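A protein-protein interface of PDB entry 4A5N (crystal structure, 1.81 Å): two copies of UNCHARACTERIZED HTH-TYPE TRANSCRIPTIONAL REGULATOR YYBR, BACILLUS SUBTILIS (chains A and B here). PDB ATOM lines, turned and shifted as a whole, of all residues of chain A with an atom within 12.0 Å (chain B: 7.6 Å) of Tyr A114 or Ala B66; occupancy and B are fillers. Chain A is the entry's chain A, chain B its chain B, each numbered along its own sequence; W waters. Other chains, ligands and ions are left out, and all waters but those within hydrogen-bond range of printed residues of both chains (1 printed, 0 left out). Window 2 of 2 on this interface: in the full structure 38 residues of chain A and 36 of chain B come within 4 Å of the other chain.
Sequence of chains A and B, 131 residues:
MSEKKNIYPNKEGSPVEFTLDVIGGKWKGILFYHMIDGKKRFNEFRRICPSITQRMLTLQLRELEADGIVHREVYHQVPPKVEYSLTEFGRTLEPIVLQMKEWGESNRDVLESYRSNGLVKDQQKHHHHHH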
ATOM      1  N   TRP A 103      25.803   3.981 -34.802  1.00  0.00           N
ATOM      2  CA  TRP A 103      25.474   2.715 -34.175  1.00  0.00           C
ATOM      3  C   TRP A 103      24.241   2.865 -33.297  1.00  0.00           C
ATOM      4  O   TRP A 103      23.337   2.032 -33.333  1.00  0.00           O
ATOM      5  CB  TRP A 103      26.686   2.227 -33.352  1.00  0.00           C
ATOM      6  CG  TRP A 103      26.513   0.818 -32.832  1.00  0.00           C
ATOM      7  CD1 TRP A 103      26.963  -0.374 -33.428  1.00  0.00           C
ATOM      8  CD2 TRP A 103      25.792   0.389 -31.625  1.00  0.00           C
ATOM      9  NE1 TRP A 103      26.570  -1.483 -32.678  1.00  0.00           N
ATOM     10  CE2 TRP A 103      25.873  -1.082 -31.586  1.00  0.00           C
ATOM     11  CE3 TRP A 103      25.073   1.049 -30.632  1.00  0.00           C
ATOM     12  CZ2 TRP A 103      25.296  -1.825 -30.562  1.00  0.00           C
ATOM     13  CZ3 TRP A 103      24.504   0.290 -29.593  1.00  0.00           C
ATOM     14  CH2 TRP A 103      24.604  -1.120 -29.569  1.00  0.00           C
ATOM     15  N   SER A 106      21.191   3.270 -35.535  1.00  0.00           N
ATOM     16  CA  SER A 106      20.911   2.025 -36.246  1.00  0.00           C
ATOM     17  C   SER A 106      20.389   0.910 -35.362  1.00  0.00           C
ATOM     18  O   SER A 106      19.569   0.106 -35.816  1.00  0.00           O
ATOM     19  CB  SER A 106      22.161   1.507 -36.947  1.00  0.00           C
ATOM     20  OG  SER A 106      22.308   2.124 -38.198  1.00  0.00           O
ATOM     21  N   ASN A 107      20.878   0.846 -34.120  1.00  0.00           N
ATOM     22  CA  ASN A 107      20.636  -0.284 -33.239  1.00  0.00           C
ATOM     23  C   ASN A 107      19.758   0.009 -32.033  1.00  0.00           C
ATOM     24  O   ASN A 107      19.532  -0.884 -31.206  1.00  0.00           O
ATOM     25  CB  ASN A 107      21.959  -0.896 -32.832  1.00  0.00           C
ATOM     26  CG  ASN A 107      22.692  -1.479 -34.028  1.00  0.00           C
ATOM     27  OD1 ASN A 107      22.157  -2.362 -34.690  1.00  0.00           O
ATOM     28  ND2 ASN A 107      23.842  -0.939 -34.368  1.00  0.00           N
ATOM     29  N   ARG A 108      19.230   1.233 -31.968  1.00  0.00           N
ATOM     30  CA  ARG A 108      18.313   1.661 -30.909  1.00  0.00           C
ATOM     31  C   ARG A 108      17.184   0.653 -30.671  1.00  0.00           C
ATOM     32  O   ARG A 108      16.973   0.235 -29.538  1.00  0.00           O
ATOM     33  CB  ARG A 108      17.739   3.052 -31.261  1.00  0.00           C
ATOM     34  CG  ARG A 108      16.711   3.620 -30.291  1.00  0.00           C
ATOM     35  CD  ARG A 108      16.178   4.974 -30.766  1.00  0.00           C
ATOM     36  NE  ARG A 108      15.253   4.859 -31.910  1.00  0.00           N
ATOM     37  CZ  ARG A 108      15.567   5.015 -33.208  1.00  0.00           C
ATOM     38  NH1 ARG A 108      16.808   5.307 -33.605  1.00  0.00           N
ATOM     39  NH2 ARG A 108      14.621   4.868 -34.135  1.00  0.00           N
ATOM     40  N   ASP A 109      16.473   0.269 -31.741  1.00  0.00           N
ATOM     41  CA  ASP A 109      15.336  -0.683 -31.661  1.00  0.00           C
ATOM     42  C   ASP A 109      15.710  -2.046 -31.087  1.00  0.00           C
ATOM     43  O   ASP A 109      15.087  -2.521 -30.139  1.00  0.00           O
ATOM     44  CB  ASP A 109      14.726  -0.926 -33.043  1.00  0.00           C
ATOM     45  CG  ASP A 109      14.138   0.326 -33.656  1.00  0.00           C
ATOM     46  OD1 ASP A 109      14.252   1.402 -33.045  1.00  0.00           O
ATOM     47  OD2 ASP A 109      13.554   0.228 -34.755  1.00  0.00           O
ATOM     48  N   VAL A 110      16.712  -2.688 -31.674  1.00  0.00           N
ATOM     49  CA  VAL A 110      17.163  -3.995 -31.183  1.00  0.00           C
ATOM     50  C   VAL A 110      17.573  -3.947 -29.723  1.00  0.00           C
ATOM     51  O   VAL A 110      17.273  -4.861 -28.960  1.00  0.00           O
ATOM     52  CB  VAL A 110      18.311  -4.569 -32.033  1.00  0.00           C
ATOM     53  CG1 VAL A 110      18.934  -5.770 -31.334  1.00  0.00           C
ATOM     54  CG2 VAL A 110      17.777  -4.988 -33.397  1.00  0.00           C
ATOM     55  N   LEU A 111      18.256  -2.874 -29.331  1.00  0.00           N
ATOM     56  CA  LEU A 111      18.777  -2.740 -27.982  1.00  0.00           C
ATOM     57  C   LEU A 111      17.665  -2.571 -26.947  1.00  0.00           C
ATOM     58  O   LEU A 111      17.664  -3.237 -25.896  1.00  0.00           O
ATOM     59  CB  LEU A 111      19.727  -1.546 -27.920  1.00  0.00           C
ATOM     60  CG  LEU A 111      20.702  -1.469 -26.752  1.00  0.00           C
ATOM     61  CD1 LEU A 111      21.144  -2.821 -26.243  1.00  0.00           C
ATOM     62  CD2 LEU A 111      21.910  -0.694 -27.227  1.00  0.00           C
ATOM     63  N   GLU A 112      16.708  -1.698 -27.255  1.00  0.00           N
ATOM     64  CA  GLU A 112      15.524  -1.552 -26.416  1.00  0.00           C
ATOM     65  C   GLU A 112      14.655  -2.830 -26.344  1.00  0.00           C
ATOM     66  O   GLU A 112      14.088  -3.120 -25.297  1.00  0.00           O
ATOM     67  CB  GLU A 112      14.711  -0.333 -26.850  1.00  0.00           C
ATOM     68  CG  GLU A 112      15.430   0.969 -26.504  1.00  0.00           C
ATOM     69  CD  GLU A 112      14.692   2.212 -26.970  1.00  0.00           C
ATOM     70  OE1 GLU A 112      13.614   2.079 -27.593  1.00  0.00           O
ATOM     71  OE2 GLU A 112      15.194   3.332 -26.705  1.00  0.00           O
ATOM     72  N   SER A 113      14.583  -3.610 -27.422  1.00  0.00           N
ATOM     73  CA  SER A 113      13.868  -4.893 -27.384  1.00  0.00           C
ATOM     74  C   SER A 113      14.576  -5.934 -26.484  1.00  0.00           C
ATOM     75  O   SER A 113      13.902  -6.753 -25.847  1.00  0.00           O
ATOM     76  CB  SER A 113      13.614  -5.447 -28.797  1.00  0.00           C
ATOM     77  OG  SER A 113      14.818  -5.715 -29.487  1.00  0.00           O
ATOM     78  N   TYR A 114      15.920  -5.894 -26.421  1.00  0.00           N
ATOM     79  CA  TYR A 114      16.682  -6.717 -25.450  1.00  0.00           C
ATOM     80  C   TYR A 114      16.435  -6.242 -24.013  1.00  0.00           C
ATOM     81  O   TYR A 114      16.353  -7.062 -23.094  1.00  0.00           O
ATOM     82  CB  TYR A 114      18.203  -6.769 -25.749  1.00  0.00           C
ATOM     83  CG  TYR A 114      18.613  -7.835 -26.765  1.00  0.00           C
ATOM     84  CD1 TYR A 114      18.488  -9.193 -26.477  1.00  0.00           C
ATOM     85  CD2 TYR A 114      19.101  -7.479 -28.013  1.00  0.00           C
ATOM     86  CE1 TYR A 114      18.842 -10.155 -27.406  1.00  0.00           C
ATOM     87  CE2 TYR A 114      19.464  -8.432 -28.942  1.00  0.00           C
ATOM     88  CZ  TYR A 114      19.322  -9.763 -28.644  1.00  0.00           C
ATOM     89  OH  TYR A 114      19.678 -10.694 -29.587  1.00  0.00           O
ATOM     90  N   ARG A 115      16.276  -4.929 -23.843  1.00  0.00           N
ATOM     91  CA  ARG A 115      16.007  -4.322 -22.528  1.00  0.00           C
ATOM     92  C   ARG A 115      14.540  -4.417 -22.056  1.00  0.00           C
ATOM     93  O   ARG A 115      14.140  -3.724 -21.121  1.00  0.00           O
ATOM     94  CB  ARG A 115      16.476  -2.851 -22.520  1.00  0.00           C
ATOM     95  CG  ARG A 115      17.982  -2.678 -22.479  1.00  0.00           C
ATOM     96  CD  ARG A 115      18.398  -1.217 -22.299  1.00  0.00           C
ATOM     97  NE  ARG A 115      19.848  -1.011 -22.463  1.00  0.00           N
ATOM     98  CZ  ARG A 115      20.520   0.107 -22.146  1.00  0.00           C
ATOM     99  NH1 ARG A 115      19.891   1.147 -21.620  1.00  0.00           N
ATOM    100  NH2 ARG A 115      21.843   0.192 -22.339  1.00  0.00           N
ATOM    101  N   SER A 116      13.739  -5.275 -22.685  1.00  0.00           N
ATOM    102  CA  SER A 116      12.371  -5.544 -22.224  1.00  0.00           C
ATOM    103  C   SER A 116      11.862  -6.868 -22.783  1.00  0.00           C
ATOM    104  O   SER A 116      11.707  -7.844 -22.047  1.00  0.00           O
ATOM    105  CB  SER A 116      11.435  -4.398 -22.623  1.00  0.00           C
ATOM    106  OG  SER A 116      11.813  -3.848 -23.876  1.00  0.00           O
ATOM    107  N   LEU B  59      28.140  -7.920 -12.204  1.00  0.00           N
ATOM    108  CA  LEU B  59      27.151  -6.896 -12.559  1.00  0.00           C
ATOM    109  C   LEU B  59      27.414  -6.348 -13.943  1.00  0.00           C
ATOM    110  O   LEU B  59      26.476  -6.258 -14.763  1.00  0.00           O
ATOM    111  CB  LEU B  59      27.145  -5.767 -11.524  1.00  0.00           C
ATOM    112  CG  LEU B  59      26.204  -4.550 -11.617  1.00  0.00           C
ATOM    113  CD1 LEU B  59      24.788  -4.943 -12.063  1.00  0.00           C
ATOM    114  CD2 LEU B  59      26.175  -3.870 -10.243  1.00  0.00           C
ATOM    115  N   GLN B  60      28.682  -6.011 -14.223  1.00  0.00           N
ATOM    116  CA  GLN B  60      29.028  -5.494 -15.557  1.00  0.00           C
ATOM    117  C   GLN B  60      28.711  -6.519 -16.640  1.00  0.00           C
ATOM    118  O   GLN B  60      28.190  -6.174 -17.722  1.00  0.00           O
ATOM    119  CB  GLN B  60      30.519  -5.087 -15.652  1.00  0.00           C
ATOM    120  CG  GLN B  60      30.931  -3.926 -14.750  1.00  0.00           C
ATOM    121  CD  GLN B  60      30.266  -2.620 -15.130  1.00  0.00           C
ATOM    122  OE1 GLN B  60      30.484  -2.084 -16.213  1.00  0.00           O
ATOM    123  NE2 GLN B  60      29.404  -2.139 -14.265  1.00  0.00           N
ATOM    124  N   LEU B  61      29.035  -7.781 -16.371  1.00  0.00           N
ATOM    125  CA  LEU B  61      28.761  -8.838 -17.360  1.00  0.00           C
ATOM    126  C   LEU B  61      27.241  -9.073 -17.538  1.00  0.00           C
ATOM    127  O   LEU B  61      26.801  -9.341 -18.635  1.00  0.00           O
ATOM    128  CB  LEU B  61      29.499 -10.150 -17.000  1.00  0.00           C
ATOM    129  CG  LEU B  61      31.021 -10.184 -17.184  1.00  0.00           C
ATOM    130  CD1 LEU B  61      31.654 -11.348 -16.406  1.00  0.00           C
ATOM    131  CD2 LEU B  61      31.411 -10.238 -18.668  1.00  0.00           C
ATOM    132  N   ARG B  62      26.468  -8.979 -16.457  1.00  0.00           N
ATOM    133  CA  ARG B  62      25.001  -9.135 -16.513  1.00  0.00           C
ATOM    134  C   ARG B  62      24.378  -8.028 -17.365  1.00  0.00           C
ATOM    135  O   ARG B  62      23.447  -8.272 -18.153  1.00  0.00           O
ATOM    136  CB  ARG B  62      24.361  -9.131 -15.094  1.00  0.00           C
ATOM    137  CG  ARG B  62      24.320 -10.493 -14.407  1.00  0.00           C
ATOM    138  CD  ARG B  62      23.508 -10.443 -13.109  1.00  0.00           C
ATOM    139  NE  ARG B  62      23.132 -11.776 -12.618  1.00  0.00           N
ATOM    140  CZ  ARG B  62      21.880 -12.246 -12.507  1.00  0.00           C
ATOM    141  NH1 ARG B  62      20.813 -11.501 -12.826  1.00  0.00           N
ATOM    142  NH2 ARG B  62      21.684 -13.485 -12.055  1.00  0.00           N
ATOM    143  N   GLU B  63      24.885  -6.808 -17.220  1.00  0.00           N
ATOM    144  CA  GLU B  63      24.369  -5.699 -18.015  1.00  0.00           C
ATOM    145  C   GLU B  63      24.688  -5.857 -19.495  1.00  0.00           C
ATOM    146  O   GLU B  63      23.830  -5.647 -20.327  1.00  0.00           O
ATOM    147  CB  GLU B  63      24.911  -4.362 -17.533  1.00  0.00           C
ATOM    148  CG  GLU B  63      24.572  -4.074 -16.091  1.00  0.00           C
ATOM    149  CD  GLU B  63      24.923  -2.674 -15.694  1.00  0.00           C
ATOM    150  OE1 GLU B  63      25.549  -1.979 -16.513  1.00  0.00           O
ATOM    151  OE2 GLU B  63      24.576  -2.275 -14.544  1.00  0.00           O
ATOM    152  N   LEU B  64      25.920  -6.226 -19.829  1.00  0.00           N
ATOM    153  CA  LEU B  64      26.278  -6.552 -21.254  1.00  0.00           C
ATOM    154  C   LEU B  64      25.418  -7.664 -21.845  1.00  0.00           C
ATOM    155  O   LEU B  64      24.952  -7.608 -23.032  1.00  0.00           O
ATOM    156  CB  LEU B  64      27.742  -6.965 -21.318  1.00  0.00           C
ATOM    157  CG  LEU B  64      28.713  -5.784 -21.315  1.00  0.00           C
ATOM    158  CD1 LEU B  64      30.134  -6.290 -21.066  1.00  0.00           C
ATOM    159  CD2 LEU B  64      28.634  -4.985 -22.612  1.00  0.00           C
ATOM    160  N   GLU B  65      25.187  -8.691 -21.027  1.00  0.00           N
ATOM    161  CA  GLU B  65      24.242  -9.767 -21.386  1.00  0.00           C
ATOM    162  C   GLU B  65      22.811  -9.256 -21.565  1.00  0.00           C
ATOM    163  O   GLU B  65      22.117  -9.583 -22.570  1.00  0.00           O
ATOM    164  CB  GLU B  65      24.306 -10.941 -20.378  1.00  0.00           C
ATOM    165  CG  GLU B  65      23.385 -12.114 -20.735  1.00  0.00           C
ATOM    166  CD  GLU B  65      23.354 -13.214 -19.671  1.00  0.00           C
ATOM    167  OE1 GLU B  65      24.003 -13.071 -18.607  1.00  0.00           O
ATOM    168  OE2 GLU B  65      22.680 -14.227 -19.916  1.00  0.00           O
ATOM    169  N   ALA B  66      22.346  -8.438 -20.618  1.00  0.00           N
ATOM    170  CA  ALA B  66      20.979  -7.940 -20.678  1.00  0.00           C
ATOM    171  C   ALA B  66      20.749  -7.085 -21.937  1.00  0.00           C
ATOM    172  O   ALA B  66      19.652  -7.074 -22.457  1.00  0.00           O
ATOM    173  CB  ALA B  66      20.627  -7.148 -19.428  1.00  0.00           C
ATOM    174  N   ASP B  67      21.792  -6.389 -22.399  1.00  0.00           N
ATOM    175  CA  ASP B  67      21.728  -5.526 -23.553  1.00  0.00           C
ATOM    176  C   ASP B  67      21.950  -6.311 -24.854  1.00  0.00           C
ATOM    177  O   ASP B  67      21.957  -5.713 -25.914  1.00  0.00           O
ATOM    178  CB  ASP B  67      22.795  -4.411 -23.465  1.00  0.00           C
ATOM    179  CG  ASP B  67      22.451  -3.324 -22.444  1.00  0.00           C
ATOM    180  OD1 ASP B  67      21.306  -3.304 -21.948  1.00  0.00           O
ATOM    181  OD2 ASP B  67      23.323  -2.471 -22.176  1.00  0.00           O
ATOM    182  N   GLY B  68      22.164  -7.626 -24.752  1.00  0.00           N
ATOM    183  CA  GLY B  68      22.355  -8.489 -25.920  1.00  0.00           C
ATOM    184  C   GLY B  68      23.734  -8.517 -26.552  1.00  0.00           C
ATOM    185  O   GLY B  68      23.895  -9.036 -27.649  1.00  0.00           O
ATOM    186  N   ILE B  69      24.723  -7.962 -25.865  1.00  0.00           N
ATOM    187  CA  ILE B  69      26.117  -7.849 -26.352  1.00  0.00           C
ATOM    188  C   ILE B  69      26.993  -9.046 -26.003  1.00  0.00           C
ATOM    189  O   ILE B  69      27.926  -9.427 -26.750  1.00  0.00           O
ATOM    190  CB  ILE B  69      26.781  -6.609 -25.710  1.00  0.00           C
ATOM    191  CG1 ILE B  69      25.891  -5.358 -25.873  1.00  0.00           C
ATOM    192  CG2 ILE B  69      28.199  -6.391 -26.255  1.00  0.00           C
ATOM    193  CD1 ILE B  69      25.554  -4.975 -27.303  1.00  0.00           C
ATOM    194  N   VAL B  70      26.653  -9.673 -24.893  1.00  0.00           N
ATOM    195  CA  VAL B  70      27.352 -10.834 -24.414  1.00  0.00           C
ATOM    196  C   VAL B  70      26.419 -12.018 -24.200  1.00  0.00           C
ATOM    197  O   VAL B  70      25.259 -11.867 -23.783  1.00  0.00           O
ATOM    198  CB  VAL B  70      28.132 -10.493 -23.127  1.00  0.00           C
ATOM    199  CG1 VAL B  70      28.642 -11.751 -22.416  1.00  0.00           C
ATOM    200  CG2 VAL B  70      29.285  -9.572 -23.482  1.00  0.00           C
ATOM    201  N   THR B  87      28.123 -11.755 -28.696  1.00  0.00           N
ATOM    202  CA  THR B  87      27.073 -12.161 -29.602  1.00  0.00           C
ATOM    203  C   THR B  87      27.394 -11.530 -30.958  1.00  0.00           C
ATOM    204  O   THR B  87      28.211 -10.596 -31.045  1.00  0.00           O
ATOM    205  CB  THR B  87      25.718 -11.636 -29.101  1.00  0.00           C
ATOM    206  OG1 THR B  87      25.720 -10.202 -29.094  1.00  0.00           O
ATOM    207  CG2 THR B  87      25.409 -12.175 -27.684  1.00  0.00           C
ATOM    208  N   GLU B  88      26.740 -11.997 -32.007  1.00  0.00           N
ATOM    209  CA  GLU B  88      26.818 -11.331 -33.289  1.00  0.00           C
ATOM    210  C   GLU B  88      26.439  -9.837 -33.207  1.00  0.00           C
ATOM    211  O   GLU B  88      27.075  -9.006 -33.819  1.00  0.00           O
ATOM    212  CB  GLU B  88      25.971 -12.074 -34.343  1.00  0.00           C
ATOM    213  CG  GLU B  88      26.595 -13.410 -34.750  1.00  0.00           C
ATOM    214  CD  GLU B  88      28.116 -13.326 -35.001  1.00  0.00           C
ATOM    215  OE1 GLU B  88      28.551 -12.581 -35.924  1.00  0.00           O
ATOM    216  OE2 GLU B  88      28.893 -13.982 -34.248  1.00  0.00           O
ATOM    217  N   PHE B  89      25.428  -9.505 -32.422  1.00  0.00           N
ATOM    218  CA  PHE B  89      25.034  -8.132 -32.216  1.00  0.00           C
ATOM    219  C   PHE B  89      26.181  -7.370 -31.514  1.00  0.00           C
ATOM    220  O   PHE B  89      26.620  -6.290 -31.936  1.00  0.00           O
ATOM    221  CB  PHE B  89      23.799  -8.118 -31.343  1.00  0.00           C
ATOM    222  CG  PHE B  89      23.254  -6.757 -31.090  1.00  0.00           C
ATOM    223  CD1 PHE B  89      22.960  -5.894 -32.146  1.00  0.00           C
ATOM    224  CD2 PHE B  89      23.023  -6.320 -29.792  1.00  0.00           C
ATOM    225  CE1 PHE B  89      22.449  -4.623 -31.909  1.00  0.00           C
ATOM    226  CE2 PHE B  89      22.499  -5.055 -29.558  1.00  0.00           C
ATOM    227  CZ  PHE B  89      22.209  -4.207 -30.607  1.00  0.00           C
ATOM    228  N   GLY B  90      26.689  -7.974 -30.459  1.00  0.00           N
ATOM    229  CA  GLY B  90      27.912  -7.473 -29.806  1.00  0.00           C
ATOM    230  C   GLY B  90      29.072  -7.104 -30.731  1.00  0.00           C
ATOM    231  O   GLY B  90      29.687  -6.051 -30.564  1.00  0.00           O
HETATM  232  O   HOH W   1      22.418 -10.697 -29.005  1.00  0.00           O
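Hydrophobic or aromatic side chains of chain A within 4 Å of the printed part of chain B: Trp A103, Val A110, Leu A111 and Tyr A114. Hydrophobic or aromatic side chains of chain B within 4 Å of the printed part of chain A: Phe B89. Along chain B the printed residues that touch a printed residue of chain A span positions 66 to 89. Among the printed residues, 8 pairs touch across the chains.
Water W1 lies within hydrogen-bond range of the backbone carbonyl oxygen of Gly B68 (2.6 Å), the side-chain hydroxyl of Tyr A114 (2.8 Å) and the side-chain hydroxyl of Thr B87 (3.3 Å).
No position is printed for both chains. Of the 8 pairs that touch across the chains among the printed residues, none has its exchanged pair printed and touching as well.
Among the printed residues, merely in contact across the chains: Trp A103 with Phe B89 (3.9 Å), Asn A107 with Phe B89 (3.6 Å), Val A110 with Phe B89 (3.7 Å), Leu A111 with Asp B67 (3.0 Å), Tyr A114 with Asp B67 (3.9 Å) and Tyr A114 with Gly B68 (3.9 Å).
O of Tyr A114 lies close to O of Ala B66 (3.4 Å). The guanidinium group (NE) of Arg A115 lies within salt-bridge range of the side-chain carboxylate (OD1) of Asp B67, at 2.8 Å.
Of chain B, only Ala B66, Asp B67 and Gly B68 come within 4 Å of Tyr A114. Of chain A, only Tyr A114 comes within 4 Å of Ala B66. No residue of chain A comes within 4 Å of Glu B63. No residue of chain A comes within 4 Å of Glu B65. Of chain A, only Leu A111, Tyr A114 and Arg A115 come within 4 Å of Asp B67. Gly B68 touches just one residue of chain A: Tyr A114 (3.9 Å). Of the printed residues of chain B, Arg A115 touches Asp B67. Of the printed residues of chain B, Trp A103 touches Phe B89 (3.9 Å). The nearest residue of chain B that does not touch Tyr A114 is Phe B89 (4.2 Å).
O of Trp A103 lies within hydrogen-bond range of ND2 of Asn A107, at 3.2 Å. The side-chain hydroxyl (OG1) of Thr B87 sits at hydrogen-bond distance from the backbone carbonyl oxygen (O) of Gly B68 (2.6 Å). OG1 of Thr B87 sits close to N of Phe B89. The side-chain hydroxyl (OG) of Ser A113 sits at hydrogen-bond distance from the backbone carbonyl oxygen (O) of Val A110 (2.7 Å).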
